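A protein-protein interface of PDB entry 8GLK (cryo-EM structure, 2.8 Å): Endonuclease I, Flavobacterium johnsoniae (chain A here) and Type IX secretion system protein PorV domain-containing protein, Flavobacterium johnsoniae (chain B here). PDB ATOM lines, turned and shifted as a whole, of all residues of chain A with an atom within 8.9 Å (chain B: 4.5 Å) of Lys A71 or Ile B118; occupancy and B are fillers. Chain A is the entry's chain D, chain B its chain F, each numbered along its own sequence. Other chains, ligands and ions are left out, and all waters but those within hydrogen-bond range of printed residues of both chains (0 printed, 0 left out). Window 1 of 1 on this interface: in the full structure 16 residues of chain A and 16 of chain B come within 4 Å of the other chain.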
ATOM      1  N   ILE A   4      28.774  11.457 -23.581  1.00  0.00           N
ATOM      2  CA  ILE A   4      27.749  11.547 -22.548  1.00  0.00           C
ATOM      3  C   ILE A   4      27.115  10.175 -22.374  1.00  0.00           C
ATOM      4  O   ILE A   4      26.563   9.611 -23.327  1.00  0.00           O
ATOM      5  CB  ILE A   4      26.690  12.603 -22.905  1.00  0.00           C
ATOM      6  CG1 ILE A   4      27.332  13.986 -23.034  1.00  0.00           C
ATOM      7  CG2 ILE A   4      25.587  12.629 -21.863  1.00  0.00           C
ATOM      8  CD1 ILE A   4      27.931  14.506 -21.749  1.00  0.00           C
ATOM      9  N   PHE A   5      27.186   9.639 -21.156  1.00  0.00           N
ATOM     10  CA  PHE A   5      26.563   8.365 -20.809  1.00  0.00           C
ATOM     11  C   PHE A   5      25.047   8.560 -20.812  1.00  0.00           C
ATOM     12  O   PHE A   5      24.597   9.702 -20.965  1.00  0.00           O
ATOM     13  CB  PHE A   5      27.116   7.867 -19.473  1.00  0.00           C
ATOM     14  CG  PHE A   5      28.375   7.058 -19.606  1.00  0.00           C
ATOM     15  CD1 PHE A   5      29.534   7.630 -20.105  1.00  0.00           C
ATOM     16  CD2 PHE A   5      28.399   5.724 -19.239  1.00  0.00           C
ATOM     17  CE1 PHE A   5      30.691   6.888 -20.230  1.00  0.00           C
ATOM     18  CE2 PHE A   5      29.551   4.976 -19.361  1.00  0.00           C
ATOM     19  CZ  PHE A   5      30.700   5.559 -19.857  1.00  0.00           C
ATOM     20  N   PRO A   6      24.214   7.498 -20.587  1.00  0.00           N
ATOM     21  CA  PRO A   6      22.958   7.382 -21.352  1.00  0.00           C
ATOM     22  C   PRO A   6      22.177   8.677 -21.492  1.00  0.00           C
ATOM     23  O   PRO A   6      21.768   9.286 -20.499  1.00  0.00           O
ATOM     24  CB  PRO A   6      22.158   6.324 -20.575  1.00  0.00           C
ATOM     25  CG  PRO A   6      23.082   5.779 -19.545  1.00  0.00           C
ATOM     26  CD  PRO A   6      24.074   6.839 -19.277  1.00  0.00           C
ATOM     27  N   ASN A   7      21.985   9.103 -22.740  1.00  0.00           N
ATOM     28  CA  ASN A   7      21.371  10.399 -23.018  1.00  0.00           C
ATOM     29  C   ASN A   7      19.959  10.529 -22.459  1.00  0.00           C
ATOM     30  O   ASN A   7      19.651  11.581 -21.877  1.00  0.00           O
ATOM     31  CB  ASN A   7      21.402  10.661 -24.530  1.00  0.00           C
ATOM     32  CG  ASN A   7      21.400  12.137 -24.866  1.00  0.00           C
ATOM     33  OD1 ASN A   7      20.375  12.808 -24.756  1.00  0.00           O
ATOM     34  ND2 ASN A   7      22.550  12.651 -25.282  1.00  0.00           N
ATOM     35  N   PRO A   8      19.062   9.540 -22.595  1.00  0.00           N
ATOM     36  CA  PRO A   8      17.770   9.668 -21.889  1.00  0.00           C
ATOM     37  C   PRO A   8      17.860   9.149 -20.458  1.00  0.00           C
ATOM     38  O   PRO A   8      17.283   8.123 -20.082  1.00  0.00           O
ATOM     39  CB  PRO A   8      16.826   8.832 -22.766  1.00  0.00           C
ATOM     40  CG  PRO A   8      17.624   8.439 -23.994  1.00  0.00           C
ATOM     41  CD  PRO A   8      19.034   8.415 -23.541  1.00  0.00           C
ATOM     42  N   PHE A  13      23.976  10.821 -14.700  1.00  0.00           N
ATOM     43  CA  PHE A  13      24.676  10.381 -15.903  1.00  0.00           C
ATOM     44  C   PHE A  13      26.178  10.482 -15.673  1.00  0.00           C
ATOM     45  O   PHE A  13      26.640  10.678 -14.549  1.00  0.00           O
ATOM     46  CB  PHE A  13      24.222  11.173 -17.138  1.00  0.00           C
ATOM     47  CG  PHE A  13      24.503  12.648 -17.065  1.00  0.00           C
ATOM     48  CD1 PHE A  13      23.627  13.503 -16.416  1.00  0.00           C
ATOM     49  CD2 PHE A  13      25.630  13.182 -17.667  1.00  0.00           C
ATOM     50  CE1 PHE A  13      23.879  14.860 -16.355  1.00  0.00           C
ATOM     51  CE2 PHE A  13      25.886  14.538 -17.610  1.00  0.00           C
ATOM     52  CZ  PHE A  13      25.010  15.377 -16.954  1.00  0.00           C
ATOM     53  N   PHE A  29      22.293  23.781 -18.489  1.00  0.00           N
ATOM     54  CA  PHE A  29      21.330  24.840 -18.733  1.00  0.00           C
ATOM     55  C   PHE A  29      19.972  24.226 -19.045  1.00  0.00           C
ATOM     56  O   PHE A  29      19.882  23.207 -19.736  1.00  0.00           O
ATOM     57  CB  PHE A  29      21.764  25.699 -19.922  1.00  0.00           C
ATOM     58  CG  PHE A  29      23.139  26.284 -19.789  1.00  0.00           C
ATOM     59  CD1 PHE A  29      23.336  27.505 -19.171  1.00  0.00           C
ATOM     60  CD2 PHE A  29      24.231  25.637 -20.346  1.00  0.00           C
ATOM     61  CE1 PHE A  29      24.601  28.051 -19.079  1.00  0.00           C
ATOM     62  CE2 PHE A  29      25.499  26.175 -20.248  1.00  0.00           C
ATOM     63  CZ  PHE A  29      25.683  27.384 -19.615  1.00  0.00           C
ATOM     64  N   PHE A  31      15.957  24.539 -20.673  1.00  0.00           N
ATOM     65  CA  PHE A  31      15.409  25.067 -21.918  1.00  0.00           C
ATOM     66  C   PHE A  31      15.029  26.535 -21.781  1.00  0.00           C
ATOM     67  O   PHE A  31      14.961  27.252 -22.785  1.00  0.00           O
ATOM     68  CB  PHE A  31      14.194  24.252 -22.360  1.00  0.00           C
ATOM     69  CG  PHE A  31      13.642  24.670 -23.695  1.00  0.00           C
ATOM     70  CD1 PHE A  31      14.210  24.204 -24.868  1.00  0.00           C
ATOM     71  CD2 PHE A  31      12.573  25.546 -23.778  1.00  0.00           C
ATOM     72  CE1 PHE A  31      13.711  24.590 -26.097  1.00  0.00           C
ATOM     73  CE2 PHE A  31      12.069  25.936 -25.005  1.00  0.00           C
ATOM     74  CZ  PHE A  31      12.640  25.457 -26.165  1.00  0.00           C
ATOM     75  N   GLY A  55      12.915  17.112 -19.075  1.00  0.00           N
ATOM     76  CA  GLY A  55      13.027  17.923 -20.272  1.00  0.00           C
ATOM     77  C   GLY A  55      14.403  17.775 -20.886  1.00  0.00           C
ATOM     78  O   GLY A  55      15.225  16.976 -20.450  1.00  0.00           O
ATOM     79  N   ILE A  56      14.637  18.564 -21.923  1.00  0.00           N
ATOM     80  CA  ILE A  56      15.942  18.594 -22.571  1.00  0.00           C
ATOM     81  C   ILE A  56      16.801  19.649 -21.891  1.00  0.00           C
ATOM     82  O   ILE A  56      16.308  20.699 -21.460  1.00  0.00           O
ATOM     83  CB  ILE A  56      15.815  18.858 -24.084  1.00  0.00           C
ATOM     84  CG1 ILE A  56      15.364  20.294 -24.351  1.00  0.00           C
ATOM     85  CG2 ILE A  56      14.858  17.862 -24.720  1.00  0.00           C
ATOM     86  CD1 ILE A  56      15.762  20.802 -25.712  1.00  0.00           C
ATOM     87  N   TYR A  57      18.092  19.357 -21.771  1.00  0.00           N
ATOM     88  CA  TYR A  57      19.038  20.252 -21.127  1.00  0.00           C
ATOM     89  C   TYR A  57      20.287  20.372 -21.986  1.00  0.00           C
ATOM     90  O   TYR A  57      20.631  19.463 -22.746  1.00  0.00           O
ATOM     91  CB  TYR A  57      19.404  19.762 -19.722  1.00  0.00           C
ATOM     92  CG  TYR A  57      18.272  19.900 -18.729  1.00  0.00           C
ATOM     93  CD1 TYR A  57      17.348  18.878 -18.554  1.00  0.00           C
ATOM     94  CD2 TYR A  57      18.120  21.056 -17.979  1.00  0.00           C
ATOM     95  CE1 TYR A  57      16.310  19.003 -17.652  1.00  0.00           C
ATOM     96  CE2 TYR A  57      17.086  21.191 -17.076  1.00  0.00           C
ATOM     97  CZ  TYR A  57      16.184  20.162 -16.916  1.00  0.00           C
ATOM     98  OH  TYR A  57      15.152  20.293 -16.016  1.00  0.00           O
ATOM     99  N   ILE A  58      20.959  21.512 -21.864  1.00  0.00           N
ATOM    100  CA  ILE A  58      22.153  21.809 -22.645  1.00  0.00           C
ATOM    101  C   ILE A  58      23.366  21.698 -21.735  1.00  0.00           C
ATOM    102  O   ILE A  58      23.448  22.382 -20.709  1.00  0.00           O
ATOM    103  CB  ILE A  58      22.069  23.205 -23.283  1.00  0.00           C
ATOM    104  CG1 ILE A  58      20.978  23.236 -24.355  1.00  0.00           C
ATOM    105  CG2 ILE A  58      23.410  23.600 -23.877  1.00  0.00           C
ATOM    106  CD1 ILE A  58      21.160  22.202 -25.441  1.00  0.00           C
ATOM    107  N   VAL A  59      24.310  20.841 -22.108  1.00  0.00           N
ATOM    108  CA  VAL A  59      25.541  20.640 -21.357  1.00  0.00           C
ATOM    109  C   VAL A  59      26.670  21.312 -22.122  1.00  0.00           C
ATOM    110  O   VAL A  59      26.940  20.966 -23.280  1.00  0.00           O
ATOM    111  CB  VAL A  59      25.836  19.148 -21.137  1.00  0.00           C
ATOM    112  CG1 VAL A  59      27.110  18.975 -20.325  1.00  0.00           C
ATOM    113  CG2 VAL A  59      24.663  18.472 -20.451  1.00  0.00           C
ATOM    114  N   LYS A  60      27.322  22.278 -21.481  1.00  0.00           N
ATOM    115  CA  LYS A  60      28.514  22.914 -22.015  1.00  0.00           C
ATOM    116  C   LYS A  60      29.724  22.358 -21.280  1.00  0.00           C
ATOM    117  O   LYS A  60      29.774  22.387 -20.043  1.00  0.00           O
ATOM    118  CB  LYS A  60      28.475  24.432 -21.858  1.00  0.00           C
ATOM    119  CG  LYS A  60      29.703  25.102 -22.460  1.00  0.00           C
ATOM    120  CD  LYS A  60      29.626  26.611 -22.419  1.00  0.00           C
ATOM    121  CE  LYS A  60      29.833  27.088 -20.996  1.00  0.00           C
ATOM    122  NZ  LYS A  60      29.894  28.565 -20.867  1.00  0.00           N
ATOM    123  N   THR A  68      32.380  22.765 -26.062  1.00  0.00           N
ATOM    124  CA  THR A  68      31.476  21.768 -26.623  1.00  0.00           C
ATOM    125  C   THR A  68      30.086  21.938 -26.030  1.00  0.00           C
ATOM    126  O   THR A  68      29.943  22.121 -24.818  1.00  0.00           O
ATOM    127  CB  THR A  68      31.999  20.352 -26.365  1.00  0.00           C
ATOM    128  OG1 THR A  68      33.286  20.209 -26.977  1.00  0.00           O
ATOM    129  CG2 THR A  68      31.054  19.311 -26.946  1.00  0.00           C
ATOM    130  N   ILE A  69      29.070  21.877 -26.886  1.00  0.00           N
ATOM    131  CA  ILE A  69      27.673  21.976 -26.477  1.00  0.00           C
ATOM    132  C   ILE A  69      26.964  20.704 -26.920  1.00  0.00           C
ATOM    133  O   ILE A  69      26.987  20.353 -28.106  1.00  0.00           O
ATOM    134  CB  ILE A  69      26.994  23.219 -27.073  1.00  0.00           C
ATOM    135  CG1 ILE A  69      27.551  24.491 -26.429  1.00  0.00           C
ATOM    136  CG2 ILE A  69      25.486  23.134 -26.901  1.00  0.00           C
ATOM    137  CD1 ILE A  69      26.918  24.832 -25.102  1.00  0.00           C
ATOM    138  N   LYS A  70      26.336  20.015 -25.971  1.00  0.00           N
ATOM    139  CA  LYS A  70      25.583  18.803 -26.257  1.00  0.00           C
ATOM    140  C   LYS A  70      24.201  18.890 -25.627  1.00  0.00           C
ATOM    141  O   LYS A  70      23.970  19.672 -24.702  1.00  0.00           O
ATOM    142  CB  LYS A  70      26.317  17.557 -25.749  1.00  0.00           C
ATOM    143  CG  LYS A  70      27.544  17.198 -26.568  1.00  0.00           C
ATOM    144  CD  LYS A  70      27.151  16.468 -27.843  1.00  0.00           C
ATOM    145  CE  LYS A  70      28.160  15.392 -28.204  1.00  0.00           C
ATOM    146  NZ  LYS A  70      29.380  15.967 -28.833  1.00  0.00           N
ATOM    147  N   LYS A  71      23.274  18.097 -26.150  1.00  0.00           N
ATOM    148  CA  LYS A  71      21.901  18.077 -25.668  1.00  0.00           C
ATOM    149  C   LYS A  71      21.609  16.737 -25.004  1.00  0.00           C
ATOM    150  O   LYS A  71      21.876  15.681 -25.584  1.00  0.00           O
ATOM    151  CB  LYS A  71      20.926  18.331 -26.818  1.00  0.00           C
ATOM    152  CG  LYS A  71      21.436  19.353 -27.818  1.00  0.00           C
ATOM    153  CD  LYS A  71      20.363  19.773 -28.801  1.00  0.00           C
ATOM    154  CE  LYS A  71      20.980  20.433 -30.024  1.00  0.00           C
ATOM    155  NZ  LYS A  71      21.119  21.906 -29.851  1.00  0.00           N
ATOM    156  N   ILE A  72      21.065  16.787 -23.789  1.00  0.00           N
ATOM    157  CA  ILE A  72      20.726  15.590 -23.033  1.00  0.00           C
ATOM    158  C   ILE A  72      19.240  15.623 -22.708  1.00  0.00           C
ATOM    159  O   ILE A  72      18.598  16.675 -22.720  1.00  0.00           O
ATOM    160  CB  ILE A  72      21.563  15.454 -21.745  1.00  0.00           C
ATOM    161  CG1 ILE A  72      21.240  16.594 -20.778  1.00  0.00           C
ATOM    162  CG2 ILE A  72      23.047  15.431 -22.072  1.00  0.00           C
ATOM    163  CD1 ILE A  72      21.764  16.371 -19.381  1.00  0.00           C
ATOM    164  N   ILE A  73      18.697  14.446 -22.407  1.00  0.00           N
ATOM    165  CA  ILE A  73      17.274  14.274 -22.133  1.00  0.00           C
ATOM    166  C   ILE A  73      17.125  13.716 -20.726  1.00  0.00           C
ATOM    167  O   ILE A  73      17.762  12.714 -20.383  1.00  0.00           O
ATOM    168  CB  ILE A  73      16.606  13.343 -23.157  1.00  0.00           C
ATOM    169  CG1 ILE A  73      16.743  13.920 -24.567  1.00  0.00           C
ATOM    170  CG2 ILE A  73      15.143  13.122 -22.804  1.00  0.00           C
ATOM    171  CD1 ILE A  73      17.008  12.878 -25.628  1.00  0.00           C
ATOM    172  N   ILE A  74      16.289  14.354 -19.914  1.00  0.00           N
ATOM    173  CA  ILE A  74      15.989  13.885 -18.569  1.00  0.00           C
ATOM    174  C   ILE A  74      14.525  13.470 -18.546  1.00  0.00           C
ATOM    175  O   ILE A  74      13.630  14.322 -18.622  1.00  0.00           O
ATOM    176  CB  ILE A  74      16.280  14.967 -17.519  1.00  0.00           C
ATOM    177  CG1 ILE A  74      17.751  15.384 -17.585  1.00  0.00           C
ATOM    178  CG2 ILE A  74      15.926  14.468 -16.129  1.00  0.00           C
ATOM    179  CD1 ILE A  74      18.723  14.261 -17.304  1.00  0.00           C
ATOM    180  N   ALA B  86      22.676  27.435 -27.898  1.00  0.00           N
ATOM    181  CA  ALA B  86      22.917  26.511 -28.996  1.00  0.00           C
ATOM    182  C   ALA B  86      21.940  26.798 -30.124  1.00  0.00           C
ATOM    183  O   ALA B  86      20.854  27.344 -29.909  1.00  0.00           O
ATOM    184  CB  ALA B  86      22.795  25.054 -28.539  1.00  0.00           C
ATOM    185  N   ASN B  87      22.343  26.416 -31.330  1.00  0.00           N
ATOM    186  CA  ASN B  87      21.508  26.556 -32.510  1.00  0.00           C
ATOM    187  C   ASN B  87      20.639  25.308 -32.664  1.00  0.00           C
ATOM    188  O   ASN B  87      20.589  24.446 -31.782  1.00  0.00           O
ATOM    189  CB  ASN B  87      22.372  26.801 -33.744  1.00  0.00           C
ATOM    190  CG  ASN B  87      23.026  28.167 -33.734  1.00  0.00           C
ATOM    191  OD1 ASN B  87      22.402  29.163 -33.375  1.00  0.00           O
ATOM    192  ND2 ASN B  87      24.291  28.220 -34.132  1.00  0.00           N
ATOM    193  N   ILE B  89      17.772  24.656 -32.255  1.00  0.00           N
ATOM    194  CA  ILE B  89      16.579  24.669 -31.419  1.00  0.00           C
ATOM    195  C   ILE B  89      15.781  25.896 -31.840  1.00  0.00           C
ATOM    196  O   ILE B  89      15.997  26.998 -31.328  1.00  0.00           O
ATOM    197  CB  ILE B  89      16.923  24.699 -29.927  1.00  0.00           C
ATOM    198  CG1 ILE B  89      17.837  23.528 -29.565  1.00  0.00           C
ATOM    199  CG2 ILE B  89      15.655  24.665 -29.090  1.00  0.00           C
ATOM    200  CD1 ILE B  89      18.241  23.501 -28.109  1.00  0.00           C
ATOM    201  N   PHE B 115      14.554  20.656 -32.130  1.00  0.00           N
ATOM    202  CA  PHE B 115      15.695  20.777 -31.234  1.00  0.00           C
ATOM    203  C   PHE B 115      17.015  20.435 -31.907  1.00  0.00           C
ATOM    204  O   PHE B 115      18.059  20.488 -31.251  1.00  0.00           O
ATOM    205  CB  PHE B 115      15.508  19.874 -30.011  1.00  0.00           C
ATOM    206  CG  PHE B 115      14.293  20.197 -29.197  1.00  0.00           C
ATOM    207  CD1 PHE B 115      14.119  21.458 -28.660  1.00  0.00           C
ATOM    208  CD2 PHE B 115      13.330  19.233 -28.960  1.00  0.00           C
ATOM    209  CE1 PHE B 115      13.005  21.755 -27.905  1.00  0.00           C
ATOM    210  CE2 PHE B 115      12.212  19.524 -28.206  1.00  0.00           C
ATOM    211  CZ  PHE B 115      12.049  20.786 -27.678  1.00  0.00           C
ATOM    212  N   GLY B 116      16.999  20.084 -33.186  1.00  0.00           N
ATOM    213  CA  GLY B 116      18.200  19.627 -33.847  1.00  0.00           C
ATOM    214  C   GLY B 116      18.524  18.188 -33.498  1.00  0.00           C
ATOM    215  O   GLY B 116      17.743  17.468 -32.869  1.00  0.00           O
ATOM    216  N   GLY B 117      19.712  17.766 -33.920  1.00  0.00           N
ATOM    217  CA  GLY B 117      20.131  16.398 -33.678  1.00  0.00           C
ATOM    218  C   GLY B 117      20.560  16.185 -32.237  1.00  0.00           C
ATOM    219  O   GLY B 117      21.236  17.021 -31.634  1.00  0.00           O
ATOM    220  N   ILE B 118      20.159  15.045 -31.681  1.00  0.00           N
ATOM    221  CA  ILE B 118      20.538  14.629 -30.337  1.00  0.00           C
ATOM    222  C   ILE B 118      21.081  13.211 -30.418  1.00  0.00           C
ATOM    223  O   ILE B 118      20.431  12.325 -30.983  1.00  0.00           O
ATOM    224  CB  ILE B 118      19.356  14.699 -29.352  1.00  0.00           C
ATOM    225  CG1 ILE B 118      18.769  16.111 -29.313  1.00  0.00           C
ATOM    226  CG2 ILE B 118      19.793  14.267 -27.963  1.00  0.00           C
ATOM    227  CD1 ILE B 118      17.615  16.262 -28.351  1.00  0.00           C
ATOM    228  N   GLU B 119      22.265  12.996 -29.852  1.00  0.00           N
ATOM    229  CA  GLU B 119      22.935  11.705 -29.919  1.00  0.00           C
ATOM    230  C   GLU B 119      22.641  10.898 -28.660  1.00  0.00           C
ATOM    231  O   GLU B 119      22.785  11.405 -27.543  1.00  0.00           O
ATOM    232  CB  GLU B 119      24.441  11.898 -30.092  1.00  0.00           C
ATOM    233  CG  GLU B 119      25.272  10.661 -29.815  1.00  0.00           C
ATOM    234  CD  GLU B 119      26.759  10.929 -29.933  1.00  0.00           C
ATOM    235  OE1 GLU B 119      27.141  11.851 -30.683  1.00  0.00           O
ATOM    236  OE2 GLU B 119      27.546  10.221 -29.271  1.00  0.00           O
ATOM    237  N   LEU B 120      22.232   9.645 -28.845  1.00  0.00           N
ATOM    238  CA  LEU B 120      21.910   8.738 -27.748  1.00  0.00           C
ATOM    239  C   LEU B 120      23.019   7.700 -27.661  1.00  0.00           C
ATOM    240  O   LEU B 120      23.257   6.955 -28.618  1.00  0.00           O
ATOM    241  CB  LEU B 120      20.553   8.077 -27.975  1.00  0.00           C
ATOM    242  CG  LEU B 120      19.423   9.011 -28.408  1.00  0.00           C
ATOM    243  CD1 LEU B 120      18.181   8.213 -28.754  1.00  0.00           C
ATOM    244  CD2 LEU B 120      19.121  10.039 -27.331  1.00  0.00           C
ATOM    245  N   ARG B 131      22.699   6.398 -32.112  1.00  0.00           N
ATOM    246  CA  ARG B 131      21.414   6.779 -32.680  1.00  0.00           C
ATOM    247  C   ARG B 131      21.209   8.280 -32.538  1.00  0.00           C
ATOM    248  O   ARG B 131      21.235   8.815 -31.426  1.00  0.00           O
ATOM    249  CB  ARG B 131      20.281   6.018 -31.991  1.00  0.00           C
ATOM    250  CG  ARG B 131      18.990   5.979 -32.779  1.00  0.00           C
ATOM    251  CD  ARG B 131      18.099   4.818 -32.357  1.00  0.00           C
ATOM    252  NE  ARG B 131      17.249   5.134 -31.216  1.00  0.00           N
ATOM    253  CZ  ARG B 131      17.576   4.913 -29.949  1.00  0.00           C
ATOM    254  NH1 ARG B 131      18.738   4.376 -29.618  1.00  0.00           N
ATOM    255  NH2 ARG B 131      16.710   5.232 -28.992  1.00  0.00           N
ATOM    256  N   GLU B 132      21.005   8.956 -33.664  1.00  0.00           N
ATOM    257  CA  GLU B 132      20.728  10.384 -33.674  1.00  0.00           C
ATOM    258  C   GLU B 132      19.240  10.603 -33.907  1.00  0.00           C
ATOM    259  O   GLU B 132      18.695  10.165 -34.925  1.00  0.00           O
ATOM    260  CB  GLU B 132      21.548  11.097 -34.751  1.00  0.00           C
ATOM    261  CG  GLU B 132      21.364  12.606 -34.768  1.00  0.00           C
ATOM    262  CD  GLU B 132      22.202  13.286 -35.831  1.00  0.00           C
ATOM    263  OE1 GLU B 132      22.932  12.581 -36.558  1.00  0.00           O
ATOM    264  OE2 GLU B 132      22.129  14.528 -35.940  1.00  0.00           O
ATOM    265  N   VAL B 133      18.590  11.278 -32.964  1.00  0.00           N
ATOM    266  CA  VAL B 133      17.156  11.517 -33.018  1.00  0.00           C
ATOM    267  C   VAL B 133      16.902  13.015 -32.955  1.00  0.00           C
ATOM    268  O   VAL B 133      17.642  13.765 -32.311  1.00  0.00           O
ATOM    269  CB  VAL B 133      16.403  10.790 -31.883  1.00  0.00           C
ATOM    270  CG1 VAL B 133      16.533   9.284 -32.040  1.00  0.00           C
ATOM    271  CG2 VAL B 133      16.920  11.236 -30.525  1.00  0.00           C
ATOM    272  N   PRO B 135      13.736  15.149 -31.955  1.00  0.00           N
ATOM    273  CA  PRO B 135      12.364  15.425 -31.510  1.00  0.00           C
ATOM    274  C   PRO B 135      11.862  16.721 -32.129  1.00  0.00           C
ATOM    275  O   PRO B 135      12.587  17.714 -32.199  1.00  0.00           O
ATOM    276  CB  PRO B 135      12.496  15.536 -29.987  1.00  0.00           C
ATOM    277  CG  PRO B 135      13.813  14.910 -29.655  1.00  0.00           C
ATOM    278  CD  PRO B 135      14.691  15.140 -30.836  1.00  0.00           C
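The side-chain amide nitrogen (ND2) of Asn A7 lies within hydrogen-bond range of the backbone carbonyl oxygen (O) of Glu B119 (2.6 Å).
The side-chain amino group of Lys A71 sits at hydrogen-bond distance from the backbone carbonyl oxygen of Asn B87, at 3.2 Å.
ND2 of Asn A7 is in hydrogen-bond range of O of Lys A71 (3.1 Å).
The backbone carbonyl oxygen (O) of Asn A7 sits at hydrogen-bond distance from the backbone NH (N) of Ile A73 (3.1 Å).
O of Val B133 lies within hydrogen-bond range of N of Ile B118, at 2.9 Å.
The backbone carbonyl oxygen of Arg B131 sits at hydrogen-bond distance from the backbone NH of Leu B120 (2.9 Å).
Asn A7 touches Ile B118 (OD1 to CG2, 3.6 Å).
Phe A31 touches Ile B89.
CE1 of Phe B115 touches CE1 of Phe A31 (3.4 Å).
Ile A56 touches Phe B115.
CG2 of Ile A69 touches CB of Ala B86 (3.7 Å).
NZ of Lys A71 touches CB of Ala B86, at 3.8 Å.
Ile B89 touches Lys A71.
Lys A71 touches Gly B117 (CE to O, 3.8 Å).
Lys A71 touches Ile B118.
Ile A73 touches Leu B120 (CD1 to CD2, 3.9 Å).
Ile B118 touches just these residues of chain A: Asn A7, Lys A71 and Ile A73.
Of the printed residues of chain B, Phe A31 touches Ile B89 (3.6 Å) and Phe B115 (3.4 Å).
Of the printed residues of chain A, Leu B120 touches Asn A7 (3.7 Å), Pro A8 (3.99 Å) and Ile A73 (3.9 Å).
Printed residues of chain A within 4 Å of Phe B115: Phe A31 (3.4 Å), Ile A56 (3.4 Å) and Lys A71 (3.2 Å).
Of the printed residues of chain B, Ile A56 touches Phe B115 (3.4 Å).
Of the printed residues of chain A, Ile B89 touches Phe A31 and Lys A71.
The nearest residue of chain A that does not touch Ile B118 is Ile A56 (4.8 Å).
Hydrophobic or aromatic side chains of chain A that line the printed part of chain B: Pro A8, Phe A31, Ile A56, Ile A69 and Ile A73.
Of the 13 printed residues of chain B, 8 touch a printed residue of chain A.
Hydrophobic or aromatic side chains of chain B within 4 Å of the printed part of chain A: Ala B86, Ile B89, Phe B115, Ile B118 and Leu B120.
Among the printed residues, 16 pairs touch across the chains.
Among the printed residues, no Asp or Glu carboxylate lies within 4 Å of a Lys or Arg side-chain nitrogen of the other chain.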
